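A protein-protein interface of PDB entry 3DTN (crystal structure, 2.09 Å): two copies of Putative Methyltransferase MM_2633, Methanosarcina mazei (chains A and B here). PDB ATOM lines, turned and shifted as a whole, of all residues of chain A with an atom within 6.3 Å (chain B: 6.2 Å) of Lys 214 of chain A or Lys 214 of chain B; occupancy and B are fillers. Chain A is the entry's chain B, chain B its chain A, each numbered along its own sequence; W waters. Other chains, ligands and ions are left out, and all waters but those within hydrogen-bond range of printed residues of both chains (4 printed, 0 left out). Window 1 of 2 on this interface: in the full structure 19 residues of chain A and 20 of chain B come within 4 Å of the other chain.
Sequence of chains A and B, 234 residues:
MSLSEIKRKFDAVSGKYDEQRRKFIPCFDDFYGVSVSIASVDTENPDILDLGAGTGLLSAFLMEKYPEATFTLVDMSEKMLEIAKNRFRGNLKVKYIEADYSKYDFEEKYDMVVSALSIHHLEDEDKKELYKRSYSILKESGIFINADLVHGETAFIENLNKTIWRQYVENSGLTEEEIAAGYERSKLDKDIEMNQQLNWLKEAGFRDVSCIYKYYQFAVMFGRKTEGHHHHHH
Water W3 lies within hydrogen-bond range of the side-chain carboxylate (OE2) of Glu 153 of chain A (2.6 Å) and the backbone NH (N) of Cys 211 of chain B (3.0 Å). Water W1 bridges OH of Tyr 213 of chain A (2.7 Å) and OH of Tyr 213 of chain B (2.7 Å). Water W2 lies within hydrogen-bond range of NZ of Lys 214 of chain A, OD1 of Asn 161 of chain A and OG of Ser 210 of chain B.
OE1 of Glu 153 of chain B lies within hydrogen-bond range of OG of Ser 210 of chain A (2.8 Å). The side-chain hydroxyl (OG) of Ser 210 of chain B lies within hydrogen-bond range of the side-chain carboxylate (OE1) of Glu 153 of chain A, at 2.9 Å. The backbone carbonyl oxygen (O) of Cys 211 of chain B lies within hydrogen-bond range of the side-chain amino group (NZ) of Lys 214 of chain A, at 2.8 Å. The backbone NH (N) of Tyr 216 of chain A is in hydrogen-bond range of the backbone carbonyl oxygen (O) of Ile 212 of chain B, 3.0 Å away. The side-chain amino group (NZ) of Lys 214 of chain B lies within hydrogen-bond range of the backbone carbonyl oxygen (O) of Cys 211 of chain A (2.9 Å). O of Lys 214 of chain B sits at hydrogen-bond distance from N of Lys 214 of chain A (2.9 Å). The backbone NH of Tyr 216 of chain B sits at hydrogen-bond distance from the backbone carbonyl oxygen of Ile 212 of chain A, at 2.9 Å.
Lys 214 of chain A touches four residues of chain B. Of chain A, only Cys 211 (2.9 Å), Tyr 213 (3.2 Å) and Lys 214 (2.9 Å) come within 4 Å of Lys 214 of chain B. Of the printed residues of chain B, Tyr 215 of chain A touches Ile 212 and Tyr 213. Of the printed residues of chain A, Ser 210 of chain B touches Glu 153 and Ile 157. Printed residues of chain A within 4 Å of Tyr 215 of chain B: Ile 212 and Tyr 213. His 151 of chain A touches none of the printed residues of chain B. Gln 217 of chain A touches none of the printed residues of chain B.
The backbone carbonyl oxygen of Tyr 216 of chain B is in hydrogen-bond range of the side-chain amino group of Lys 214 of chain B (2.8 Å). The backbone carbonyl oxygen (O) of Val 220 of chain A is in hydrogen-bond range of the backbone NH (N) of Ile 212 of chain A. NZ of Lys 214 of chain A is in hydrogen-bond range of O of Tyr 216 of chain A (2.8 Å).
Ile 157 of chain A touches Ser 210 of chain B, and with the chains exchanged Ser 210 of chain A touches Ile 157 of chain B. Tyr 213 of chain A touches Tyr 215 of chain B, and with the chains exchanged Tyr 215 of chain A touches Tyr 213 of chain B. 17 positions are printed for both chains. Of the 17 pairs that touch across the chains among the printed residues, 16 have their exchanged pair printed and touching as well.
Hydrophobic or aromatic side chains of chain B within 4 Å of the printed part of chain A: Ile 157, Ile 212, Tyr 213, Tyr 215 and Tyr 216. Of the 17 printed residues of chain A, 9 touch a printed residue of chain B. Among the printed residues, 17 pairs touch across the chains.
Ser 210 of chain A touches Ile 157 of chain B. Tyr 215 of chain B touches Ile 212 of chain A. CD1 of Tyr 213 of chain A touches O of Lys 214 of chain B, at 3.2 Å. O of Lys 214 of chain A touches O of Ile 212 of chain B (3.9 Å). CD1 of Tyr 213 of chain B touches O of Lys 214 of chain A, at 3.2 Å. CA of Tyr 215 of chain A touches O of Ile 212 of chain B, at 3.9 Å. Tyr 213 of chain B touches Tyr 215 of chain A (CD1 to CD1, 3.9 Å).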
ATOM      1  N   VAL A 150     -26.940 -23.577   3.313  1.00  0.00           N
ATOM      2  CA  VAL A 150     -27.490 -24.786   3.913  1.00  0.00           C
ATOM      3  C   VAL A 150     -28.327 -24.399   5.147  1.00  0.00           C
ATOM      4  O   VAL A 150     -28.119 -23.355   5.782  1.00  0.00           O
ATOM      5  CB  VAL A 150     -26.383 -25.803   4.283  1.00  0.00           C
ATOM      6  CG1 VAL A 150     -25.702 -26.336   3.008  1.00  0.00           C
ATOM      7  CG2 VAL A 150     -25.356 -25.159   5.181  1.00  0.00           C
ATOM      8  N   HIS A 151     -29.299 -25.220   5.470  1.00  0.00           N
ATOM      9  CA  HIS A 151     -30.202 -24.924   6.548  1.00  0.00           C
ATOM     10  C   HIS A 151     -29.612 -25.479   7.870  1.00  0.00           C
ATOM     11  O   HIS A 151     -28.972 -26.537   7.890  1.00  0.00           O
ATOM     12  CB  HIS A 151     -31.542 -25.640   6.277  1.00  0.00           C
ATOM     13  CG  HIS A 151     -32.688 -25.118   7.110  1.00  0.00           C
ATOM     14  ND1 HIS A 151     -33.386 -23.965   6.781  1.00  0.00           N
ATOM     15  CD2 HIS A 151     -33.260 -25.593   8.242  1.00  0.00           C
ATOM     16  CE1 HIS A 151     -34.337 -23.757   7.684  1.00  0.00           C
ATOM     17  NE2 HIS A 151     -34.275 -24.724   8.586  1.00  0.00           N
ATOM     18  N   GLU A 153     -29.311 -27.534  11.302  1.00  0.00           N
ATOM     19  CA  GLU A 153     -29.638 -28.917  11.557  1.00  0.00           C
ATOM     20  C   GLU A 153     -30.845 -29.000  12.481  1.00  0.00           C
ATOM     21  O   GLU A 153     -31.578 -29.968  12.452  1.00  0.00           O
ATOM     22  CB  GLU A 153     -28.404 -29.621  12.209  1.00  0.00           C
ATOM     23  CG  GLU A 153     -27.338 -30.073  11.190  1.00  0.00           C
ATOM     24  CD  GLU A 153     -26.452 -28.944  10.704  1.00  0.00           C
ATOM     25  OE1 GLU A 153     -26.495 -27.851  11.317  1.00  0.00           O
ATOM     26  OE2 GLU A 153     -25.688 -29.137   9.722  1.00  0.00           O
ATOM     27  N   ILE A 157     -30.145 -24.072  15.609  1.00  0.00           N
ATOM     28  CA  ILE A 157     -28.970 -23.833  14.768  1.00  0.00           C
ATOM     29  C   ILE A 157     -29.346 -22.915  13.592  1.00  0.00           C
ATOM     30  O   ILE A 157     -28.578 -22.026  13.208  1.00  0.00           O
ATOM     31  CB  ILE A 157     -28.332 -25.165  14.274  1.00  0.00           C
ATOM     32  CG1 ILE A 157     -27.801 -25.950  15.495  1.00  0.00           C
ATOM     33  CG2 ILE A 157     -27.146 -24.873  13.269  1.00  0.00           C
ATOM     34  CD1 ILE A 157     -26.631 -25.235  16.204  1.00  0.00           C
ATOM     35  N   ASN A 161     -27.489 -19.444  12.952  1.00  0.00           N
ATOM     36  CA  ASN A 161     -26.890 -19.087  11.672  1.00  0.00           C
ATOM     37  C   ASN A 161     -27.455 -17.763  11.159  1.00  0.00           C
ATOM     38  O   ASN A 161     -26.712 -16.896  10.720  1.00  0.00           O
ATOM     39  CB  ASN A 161     -27.145 -20.169  10.586  1.00  0.00           C
ATOM     40  CG  ASN A 161     -26.369 -21.485  10.817  1.00  0.00           C
ATOM     41  OD1 ASN A 161     -25.504 -21.594  11.704  1.00  0.00           O
ATOM     42  ND2 ASN A 161     -26.699 -22.504  10.002  1.00  0.00           N
ATOM     43  N   MET A 194     -27.023 -29.549   5.336  1.00  0.00           N
ATOM     44  CA  MET A 194     -25.844 -29.961   4.564  1.00  0.00           C
ATOM     45  C   MET A 194     -25.703 -31.469   4.429  1.00  0.00           C
ATOM     46  O   MET A 194     -25.446 -31.964   3.331  1.00  0.00           O
ATOM     47  CB  MET A 194     -24.573 -29.440   5.159  1.00  0.00           C
ATOM     48  CG  MET A 194     -23.362 -29.850   4.315  1.00  0.00           C
ATOM     49  SD  MET A 194     -22.035 -28.979   5.060  1.00  0.00           S
ATOM     50  CE  MET A 194     -21.797 -29.993   6.560  1.00  0.00           C
ATOM     51  N   SER A 210     -17.443 -34.575   0.492  1.00  0.00           N
ATOM     52  CA  SER A 210     -17.004 -33.868   1.684  1.00  0.00           C
ATOM     53  C   SER A 210     -17.480 -32.416   1.668  1.00  0.00           C
ATOM     54  O   SER A 210     -17.577 -31.797   0.613  1.00  0.00           O
ATOM     55  CB  SER A 210     -15.458 -33.948   1.789  1.00  0.00           C
ATOM     56  OG  SER A 210     -14.961 -33.266   2.924  1.00  0.00           O
ATOM     57  N   CYS A 211     -17.770 -31.885   2.850  1.00  0.00           N
ATOM     58  CA  CYS A 211     -17.906 -30.471   3.047  1.00  0.00           C
ATOM     59  C   CYS A 211     -16.509 -29.924   3.333  1.00  0.00           C
ATOM     60  O   CYS A 211     -15.894 -30.278   4.365  1.00  0.00           O
ATOM     61  CB  CYS A 211     -18.842 -30.212   4.259  1.00  0.00           C
ATOM     62  SG  CYS A 211     -18.752 -28.468   4.803  1.00  0.00           S
ATOM     63  N   ILE A 212     -15.968 -29.122   2.421  1.00  0.00           N
ATOM     64  CA  ILE A 212     -14.550 -28.671   2.544  1.00  0.00           C
ATOM     65  C   ILE A 212     -14.478 -27.393   3.390  1.00  0.00           C
ATOM     66  O   ILE A 212     -13.483 -27.103   4.079  1.00  0.00           O
ATOM     67  CB  ILE A 212     -13.946 -28.386   1.142  1.00  0.00           C
ATOM     68  CG1 ILE A 212     -14.315 -29.519   0.169  1.00  0.00           C
ATOM     69  CG2 ILE A 212     -12.370 -28.184   1.223  1.00  0.00           C
ATOM     70  CD1 ILE A 212     -13.487 -30.820   0.404  1.00  0.00           C
ATOM     71  N   TYR A 213     -15.536 -26.595   3.265  1.00  0.00           N
ATOM     72  CA  TYR A 213     -15.602 -25.330   3.921  1.00  0.00           C
ATOM     73  C   TYR A 213     -17.034 -25.100   4.433  1.00  0.00           C
ATOM     74  O   TYR A 213     -18.024 -25.440   3.750  1.00  0.00           O
ATOM     75  CB  TYR A 213     -15.169 -24.192   2.965  1.00  0.00           C
ATOM     76  CG  TYR A 213     -15.184 -22.835   3.680  1.00  0.00           C
ATOM     77  CD1 TYR A 213     -14.205 -22.509   4.596  1.00  0.00           C
ATOM     78  CD2 TYR A 213     -16.220 -21.895   3.465  1.00  0.00           C
ATOM     79  CE1 TYR A 213     -14.221 -21.269   5.250  1.00  0.00           C
ATOM     80  CE2 TYR A 213     -16.259 -20.689   4.135  1.00  0.00           C
ATOM     81  CZ  TYR A 213     -15.250 -20.359   4.996  1.00  0.00           C
ATOM     82  OH  TYR A 213     -15.274 -19.166   5.696  1.00  0.00           O
ATOM     83  N   LYS A 214     -17.148 -24.536   5.640  1.00  0.00           N
ATOM     84  CA  LYS A 214     -18.405 -24.215   6.215  1.00  0.00           C
ATOM     85  C   LYS A 214     -18.274 -23.000   7.122  1.00  0.00           C
ATOM     86  O   LYS A 214     -17.347 -22.903   7.903  1.00  0.00           O
ATOM     87  CB  LYS A 214     -19.025 -25.375   7.006  1.00  0.00           C
ATOM     88  CG  LYS A 214     -20.558 -25.076   7.379  1.00  0.00           C
ATOM     89  CD  LYS A 214     -21.252 -26.388   7.879  1.00  0.00           C
ATOM     90  CE  LYS A 214     -22.757 -26.178   8.117  1.00  0.00           C
ATOM     91  NZ  LYS A 214     -22.942 -25.272   9.329  1.00  0.00           N
ATOM     92  N   TYR A 215     -19.175 -22.033   6.939  1.00  0.00           N
ATOM     93  CA  TYR A 215     -19.208 -20.857   7.808  1.00  0.00           C
ATOM     94  C   TYR A 215     -20.671 -20.534   8.097  1.00  0.00           C
ATOM     95  O   TYR A 215     -21.372 -19.938   7.257  1.00  0.00           O
ATOM     96  CB  TYR A 215     -18.479 -19.689   7.127  1.00  0.00           C
ATOM     97  CG  TYR A 215     -18.428 -18.444   7.958  1.00  0.00           C
ATOM     98  CD1 TYR A 215     -17.368 -18.224   8.829  1.00  0.00           C
ATOM     99  CD2 TYR A 215     -19.438 -17.447   7.850  1.00  0.00           C
ATOM    100  CE1 TYR A 215     -17.287 -17.043   9.580  1.00  0.00           C
ATOM    101  CE2 TYR A 215     -19.368 -16.282   8.597  1.00  0.00           C
ATOM    102  CZ  TYR A 215     -18.289 -16.079   9.453  1.00  0.00           C
ATOM    103  OH  TYR A 215     -18.194 -14.938  10.219  1.00  0.00           O
ATOM    104  N   TYR A 216     -21.146 -20.978   9.252  1.00  0.00           N
ATOM    105  CA  TYR A 216     -22.585 -20.993   9.554  1.00  0.00           C
ATOM    106  C   TYR A 216     -23.388 -21.557   8.368  1.00  0.00           C
ATOM    107  O   TYR A 216     -23.247 -22.727   8.103  1.00  0.00           O
ATOM    108  CB  TYR A 216     -23.073 -19.631  10.052  1.00  0.00           C
ATOM    109  CG  TYR A 216     -22.250 -19.091  11.245  1.00  0.00           C
ATOM    110  CD1 TYR A 216     -22.641 -19.341  12.554  1.00  0.00           C
ATOM    111  CD2 TYR A 216     -21.087 -18.332  11.036  1.00  0.00           C
ATOM    112  CE1 TYR A 216     -21.880 -18.860  13.654  1.00  0.00           C
ATOM    113  CE2 TYR A 216     -20.365 -17.794  12.128  1.00  0.00           C
ATOM    114  CZ  TYR A 216     -20.782 -18.090  13.430  1.00  0.00           C
ATOM    115  OH  TYR A 216     -20.102 -17.566  14.498  1.00  0.00           O
ATOM    116  N   GLN A 217     -24.263 -20.785   7.698  1.00  0.00           N
ATOM    117  CA  GLN A 217     -25.078 -21.382   6.584  1.00  0.00           C
ATOM    118  C   GLN A 217     -24.380 -21.510   5.251  1.00  0.00           C
ATOM    119  O   GLN A 217     -24.970 -21.990   4.267  1.00  0.00           O
ATOM    120  CB  GLN A 217     -26.346 -20.552   6.309  1.00  0.00           C
ATOM    121  CG  GLN A 217     -26.070 -19.108   5.849  1.00  0.00           C
ATOM    122  CD  GLN A 217     -26.038 -18.136   7.013  1.00  0.00           C
ATOM    123  OE1 GLN A 217     -25.009 -17.992   7.702  1.00  0.00           O
ATOM    124  NE2 GLN A 217     -27.212 -17.496   7.294  1.00  0.00           N
ATOM    125  N   PHE A 218     -23.161 -21.009   5.147  1.00  0.00           N
ATOM    126  CA  PHE A 218     -22.428 -21.121   3.890  1.00  0.00           C
ATOM    127  C   PHE A 218     -21.552 -22.373   3.886  1.00  0.00           C
ATOM    128  O   PHE A 218     -20.778 -22.552   4.778  1.00  0.00           O
ATOM    129  CB  PHE A 218     -21.567 -19.881   3.724  1.00  0.00           C
ATOM    130  CG  PHE A 218     -22.368 -18.621   3.603  1.00  0.00           C
ATOM    131  CD1 PHE A 218     -22.804 -18.176   2.355  1.00  0.00           C
ATOM    132  CD2 PHE A 218     -22.680 -17.868   4.742  1.00  0.00           C
ATOM    133  CE1 PHE A 218     -23.540 -16.988   2.224  1.00  0.00           C
ATOM    134  CE2 PHE A 218     -23.419 -16.682   4.619  1.00  0.00           C
ATOM    135  CZ  PHE A 218     -23.863 -16.261   3.357  1.00  0.00           C
ATOM    136  N   ALA A 219     -21.684 -23.246   2.878  1.00  0.00           N
ATOM    137  CA  ALA A 219     -20.873 -24.488   2.837  1.00  0.00           C
ATOM    138  C   ALA A 219     -20.383 -24.761   1.406  1.00  0.00           C
ATOM    139  O   ALA A 219     -21.100 -24.460   0.429  1.00  0.00           O
ATOM    140  CB  ALA A 219     -21.727 -25.670   3.351  1.00  0.00           C
ATOM    141  N   VAL A 220     -19.171 -25.287   1.272  1.00  0.00           N
ATOM    142  CA  VAL A 220     -18.657 -25.728  -0.007  1.00  0.00           C
ATOM    143  C   VAL A 220     -18.645 -27.239   0.049  1.00  0.00           C
ATOM    144  O   VAL A 220     -17.982 -27.854   0.906  1.00  0.00           O
ATOM    145  CB  VAL A 220     -17.276 -25.118  -0.306  1.00  0.00           C
ATOM    146  CG1 VAL A 220     -16.699 -25.637  -1.651  1.00  0.00           C
ATOM    147  CG2 VAL A 220     -17.345 -23.575  -0.293  1.00  0.00           C
ATOM    148  N   VAL B 150      -9.957 -32.625  12.185  1.00  0.00           N
ATOM    149  CA  VAL B 150     -10.737 -33.788  11.768  1.00  0.00           C
ATOM    150  C   VAL B 150     -10.022 -34.458  10.607  1.00  0.00           C
ATOM    151  O   VAL B 150      -9.285 -33.828   9.863  1.00  0.00           O
ATOM    152  CB  VAL B 150     -12.188 -33.424  11.346  1.00  0.00           C
ATOM    153  CG1 VAL B 150     -12.986 -33.106  12.601  1.00  0.00           C
ATOM    154  CG2 VAL B 150     -12.201 -32.237  10.349  1.00  0.00           C
ATOM    155  N   HIS B 151     -10.245 -35.754  10.461  1.00  0.00           N
ATOM    156  CA  HIS B 151      -9.601 -36.513   9.428  1.00  0.00           C
ATOM    157  C   HIS B 151     -10.368 -36.392   8.122  1.00  0.00           C
ATOM    158  O   HIS B 151     -11.574 -36.239   8.146  1.00  0.00           O
ATOM    159  CB  HIS B 151      -9.572 -38.004   9.833  1.00  0.00           C
ATOM    160  CG  HIS B 151      -8.619 -38.818   9.014  1.00  0.00           C
ATOM    161  ND1 HIS B 151      -7.262 -38.849   9.279  1.00  0.00           N
ATOM    162  CD2 HIS B 151      -8.809 -39.613   7.927  1.00  0.00           C
ATOM    163  CE1 HIS B 151      -6.664 -39.650   8.415  1.00  0.00           C
ATOM    164  NE2 HIS B 151      -7.573 -40.126   7.582  1.00  0.00           N
ATOM    165  N   GLU B 153     -12.401 -37.482   4.817  1.00  0.00           N
ATOM    166  CA  GLU B 153     -13.408 -38.547   4.664  1.00  0.00           C
ATOM    167  C   GLU B 153     -12.868 -39.738   3.896  1.00  0.00           C
ATOM    168  O   GLU B 153     -13.385 -40.846   4.046  1.00  0.00           O
ATOM    169  CB  GLU B 153     -14.682 -37.984   3.929  1.00  0.00           C
ATOM    170  CG  GLU B 153     -15.600 -37.258   4.898  1.00  0.00           C
ATOM    171  CD  GLU B 153     -15.059 -35.848   5.274  1.00  0.00           C
ATOM    172  OE1 GLU B 153     -14.110 -35.354   4.582  1.00  0.00           O
ATOM    173  OE2 GLU B 153     -15.620 -35.221   6.231  1.00  0.00           O
ATOM    174  N   ILE B 157      -9.338 -36.904   0.178  1.00  0.00           N
ATOM    175  CA  ILE B 157      -9.688 -35.649   0.906  1.00  0.00           C
ATOM    176  C   ILE B 157      -8.649 -35.351   2.001  1.00  0.00           C
ATOM    177  O   ILE B 157      -8.247 -34.232   2.176  1.00  0.00           O
ATOM    178  CB  ILE B 157     -11.098 -35.702   1.605  1.00  0.00           C
ATOM    179  CG1 ILE B 157     -12.238 -35.854   0.577  1.00  0.00           C
ATOM    180  CG2 ILE B 157     -11.300 -34.417   2.496  1.00  0.00           C
ATOM    181  CD1 ILE B 157     -12.318 -34.602  -0.330  1.00  0.00           C
ATOM    182  N   ASN B 161      -6.533 -31.936   2.290  1.00  0.00           N
ATOM    183  CA  ASN B 161      -6.426 -31.166   3.555  1.00  0.00           C
ATOM    184  C   ASN B 161      -4.951 -30.939   3.934  1.00  0.00           C
ATOM    185  O   ASN B 161      -4.538 -29.811   4.193  1.00  0.00           O
ATOM    186  CB  ASN B 161      -7.099 -31.898   4.727  1.00  0.00           C
ATOM    187  CG  ASN B 161      -8.647 -31.992   4.615  1.00  0.00           C
ATOM    188  OD1 ASN B 161      -9.286 -31.351   3.758  1.00  0.00           O
ATOM    189  ND2 ASN B 161      -9.252 -32.761   5.536  1.00  0.00           N
ATOM    190  N   MET B 194     -15.155 -36.014  10.788  1.00  0.00           N
ATOM    191  CA  MET B 194     -16.086 -35.198  11.533  1.00  0.00           C
ATOM    192  C   MET B 194     -17.423 -35.824  11.880  1.00  0.00           C
ATOM    193  O   MET B 194     -17.919 -35.614  12.985  1.00  0.00           O
ATOM    194  CB  MET B 194     -16.361 -33.945  10.790  1.00  0.00           C
ATOM    195  CG  MET B 194     -17.356 -33.061  11.500  1.00  0.00           C
ATOM    196  SD  MET B 194     -17.306 -31.461  10.682  1.00  0.00           S
ATOM    197  CE  MET B 194     -18.335 -31.782   9.226  1.00  0.00           C
ATOM    198  N   SER B 210     -23.985 -29.742  15.628  1.00  0.00           N
ATOM    199  CA  SER B 210     -23.725 -29.184  14.314  1.00  0.00           C
ATOM    200  C   SER B 210     -22.218 -28.884  14.154  1.00  0.00           C
ATOM    201  O   SER B 210     -21.522 -28.599  15.108  1.00  0.00           O
ATOM    202  CB  SER B 210     -24.488 -27.887  14.230  1.00  0.00           C
ATOM    203  OG  SER B 210     -24.225 -27.189  13.032  1.00  0.00           O
ATOM    204  N   CYS B 211     -21.731 -28.994  12.946  1.00  0.00           N
ATOM    205  CA  CYS B 211     -20.481 -28.396  12.591  1.00  0.00           C
ATOM    206  C   CYS B 211     -20.750 -26.954  12.158  1.00  0.00           C
ATOM    207  O   CYS B 211     -21.410 -26.707  11.121  1.00  0.00           O
ATOM    208  CB  CYS B 211     -19.848 -29.142  11.441  1.00  0.00           C
ATOM    209  SG  CYS B 211     -18.398 -28.254  10.814  1.00  0.00           S
ATOM    210  N   ILE B 212     -20.256 -25.989  12.947  1.00  0.00           N
ATOM    211  CA  ILE B 212     -20.560 -24.575  12.690  1.00  0.00           C
ATOM    212  C   ILE B 212     -19.552 -23.985  11.715  1.00  0.00           C
ATOM    213  O   ILE B 212     -19.868 -23.070  10.925  1.00  0.00           O
ATOM    214  CB  ILE B 212     -20.467 -23.779  13.988  1.00  0.00           C
ATOM    215  CG1 ILE B 212     -21.259 -24.488  15.107  1.00  0.00           C
ATOM    216  CG2 ILE B 212     -20.962 -22.362  13.750  1.00  0.00           C
ATOM    217  CD1 ILE B 212     -22.736 -24.433  14.869  1.00  0.00           C
ATOM    218  N   TYR B 213     -18.306 -24.456  11.824  1.00  0.00           N
ATOM    219  CA  TYR B 213     -17.241 -23.958  11.009  1.00  0.00           C
ATOM    220  C   TYR B 213     -16.346 -25.093  10.590  1.00  0.00           C
ATOM    221  O   TYR B 213     -16.061 -26.003  11.402  1.00  0.00           O
ATOM    222  CB  TYR B 213     -16.374 -22.944  11.819  1.00  0.00           C
ATOM    223  CG  TYR B 213     -15.242 -22.377  11.005  1.00  0.00           C
ATOM    224  CD1 TYR B 213     -15.495 -21.416  10.065  1.00  0.00           C
ATOM    225  CD2 TYR B 213     -13.930 -22.871  11.122  1.00  0.00           C
ATOM    226  CE1 TYR B 213     -14.484 -20.899   9.287  1.00  0.00           C
ATOM    227  CE2 TYR B 213     -12.913 -22.356  10.333  1.00  0.00           C
ATOM    228  CZ  TYR B 213     -13.204 -21.346   9.430  1.00  0.00           C
ATOM    229  OH  TYR B 213     -12.263 -20.742   8.600  1.00  0.00           O
ATOM    230  N   LYS B 214     -15.836 -25.009   9.358  1.00  0.00           N
ATOM    231  CA  LYS B 214     -14.894 -26.006   8.849  1.00  0.00           C
ATOM    232  C   LYS B 214     -14.033 -25.336   7.795  1.00  0.00           C
ATOM    233  O   LYS B 214     -14.531 -24.527   6.998  1.00  0.00           O
ATOM    234  CB  LYS B 214     -15.613 -27.225   8.244  1.00  0.00           C
ATOM    235  CG  LYS B 214     -14.655 -28.352   7.844  1.00  0.00           C
ATOM    236  CD  LYS B 214     -15.465 -29.636   7.563  1.00  0.00           C
ATOM    237  CE  LYS B 214     -14.542 -30.877   7.477  1.00  0.00           C
ATOM    238  NZ  LYS B 214     -13.688 -30.734   6.211  1.00  0.00           N
ATOM    239  N   TYR B 215     -12.738 -25.645   7.819  1.00  0.00           N
ATOM    240  CA  TYR B 215     -11.813 -25.152   6.806  1.00  0.00           C
ATOM    241  C   TYR B 215     -10.838 -26.296   6.629  1.00  0.00           C
ATOM    242  O   TYR B 215      -9.933 -26.468   7.473  1.00  0.00           O
ATOM    243  CB  TYR B 215     -11.089 -23.915   7.352  1.00  0.00           C
ATOM    244  CG  TYR B 215     -10.102 -23.282   6.388  1.00  0.00           C
ATOM    245  CD1 TYR B 215     -10.509 -22.359   5.442  1.00  0.00           C
ATOM    246  CD2 TYR B 215      -8.748 -23.612   6.444  1.00  0.00           C
ATOM    247  CE1 TYR B 215      -9.584 -21.783   4.593  1.00  0.00           C
ATOM    248  CE2 TYR B 215      -7.820 -23.042   5.584  1.00  0.00           C
ATOM    249  CZ  TYR B 215      -8.234 -22.147   4.675  1.00  0.00           C
ATOM    250  OH  TYR B 215      -7.306 -21.597   3.840  1.00  0.00           O
ATOM    251  N   TYR B 216     -11.062 -27.130   5.605  1.00  0.00           N
ATOM    252  CA  TYR B 216     -10.306 -28.393   5.450  1.00  0.00           C
ATOM    253  C   TYR B 216     -10.280 -29.213   6.739  1.00  0.00           C
ATOM    254  O   TYR B 216     -11.324 -29.650   7.154  1.00  0.00           O
ATOM    255  CB  TYR B 216      -8.905 -28.162   4.884  1.00  0.00           C
ATOM    256  CG  TYR B 216      -8.939 -27.414   3.562  1.00  0.00           C
ATOM    257  CD1 TYR B 216      -8.999 -28.080   2.357  1.00  0.00           C
ATOM    258  CD2 TYR B 216      -8.881 -26.039   3.541  1.00  0.00           C
ATOM    259  CE1 TYR B 216      -8.990 -27.371   1.130  1.00  0.00           C
ATOM    260  CE2 TYR B 216      -8.879 -25.338   2.355  1.00  0.00           C
ATOM    261  CZ  TYR B 216      -8.938 -26.004   1.152  1.00  0.00           C
ATOM    262  OH  TYR B 216      -8.954 -25.270  -0.043  1.00  0.00           O
ATOM    263  N   GLN B 217      -9.110 -29.524   7.322  1.00  0.00           N
ATOM    264  CA  GLN B 217      -9.113 -30.339   8.530  1.00  0.00           C
ATOM    265  C   GLN B 217      -9.498 -29.650   9.841  1.00  0.00           C
ATOM    266  O   GLN B 217      -9.426 -30.267  10.880  1.00  0.00           O
ATOM    267  CB  GLN B 217      -7.710 -30.993   8.776  1.00  0.00           C
ATOM    268  CG  GLN B 217      -6.657 -30.007   9.081  1.00  0.00           C
ATOM    269  CD  GLN B 217      -5.943 -29.593   7.829  1.00  0.00           C
ATOM    270  OE1 GLN B 217      -6.384 -28.673   7.109  1.00  0.00           O
ATOM    271  NE2 GLN B 217      -4.838 -30.287   7.527  1.00  0.00           N
ATOM    272  N   PHE B 218      -9.756 -28.362   9.824  1.00  0.00           N
ATOM    273  CA  PHE B 218     -10.074 -27.660  11.062  1.00  0.00           C
ATOM    274  C   PHE B 218     -11.602 -27.556  11.114  1.00  0.00           C
ATOM    275  O   PHE B 218     -12.206 -27.037  10.168  1.00  0.00           O
ATOM    276  CB  PHE B 218      -9.431 -26.242  11.016  1.00  0.00           C
ATOM    277  CG  PHE B 218      -7.925 -26.280  10.996  1.00  0.00           C
ATOM    278  CD1 PHE B 218      -7.214 -26.354  12.202  1.00  0.00           C
ATOM    279  CD2 PHE B 218      -7.221 -26.294   9.798  1.00  0.00           C
ATOM    280  CE1 PHE B 218      -5.821 -26.415  12.226  1.00  0.00           C
ATOM    281  CE2 PHE B 218      -5.814 -26.412   9.823  1.00  0.00           C
ATOM    282  CZ  PHE B 218      -5.125 -26.489  11.066  1.00  0.00           C
ATOM    283  N   ALA B 219     -12.212 -27.968  12.226  1.00  0.00           N
ATOM    284  CA  ALA B 219     -13.679 -27.898  12.357  1.00  0.00           C
ATOM    285  C   ALA B 219     -14.094 -27.419  13.750  1.00  0.00           C
ATOM    286  O   ALA B 219     -13.443 -27.761  14.744  1.00  0.00           O
ATOM    287  CB  ALA B 219     -14.267 -29.287  12.117  1.00  0.00           C
ATOM    288  N   VAL B 220     -15.170 -26.648  13.846  1.00  0.00           N
ATOM    289  CA  VAL B 220     -15.644 -26.220  15.115  1.00  0.00           C
ATOM    290  C   VAL B 220     -16.952 -26.932  15.266  1.00  0.00           C
ATOM    291  O   VAL B 220     -17.877 -26.704  14.476  1.00  0.00           O
ATOM    292  CB  VAL B 220     -15.826 -24.670  15.229  1.00  0.00           C
ATOM    293  CG1 VAL B 220     -16.563 -24.339  16.552  1.00  0.00           C
ATOM    294  CG2 VAL B 220     -14.471 -23.917  15.078  1.00  0.00           C
HETATM  295  O   HOH W   1     -12.974 -18.707   6.940  1.00  0.00           O
HETATM  296  O   HOH W   2     -24.005 -24.174  11.749  1.00  0.00           O
HETATM  297  O   HOH W   3     -23.353 -29.811  10.561  1.00  0.00           O
HETATM  298  O   HOH W   4     -17.347 -33.287   5.281  1.00  0.00           O
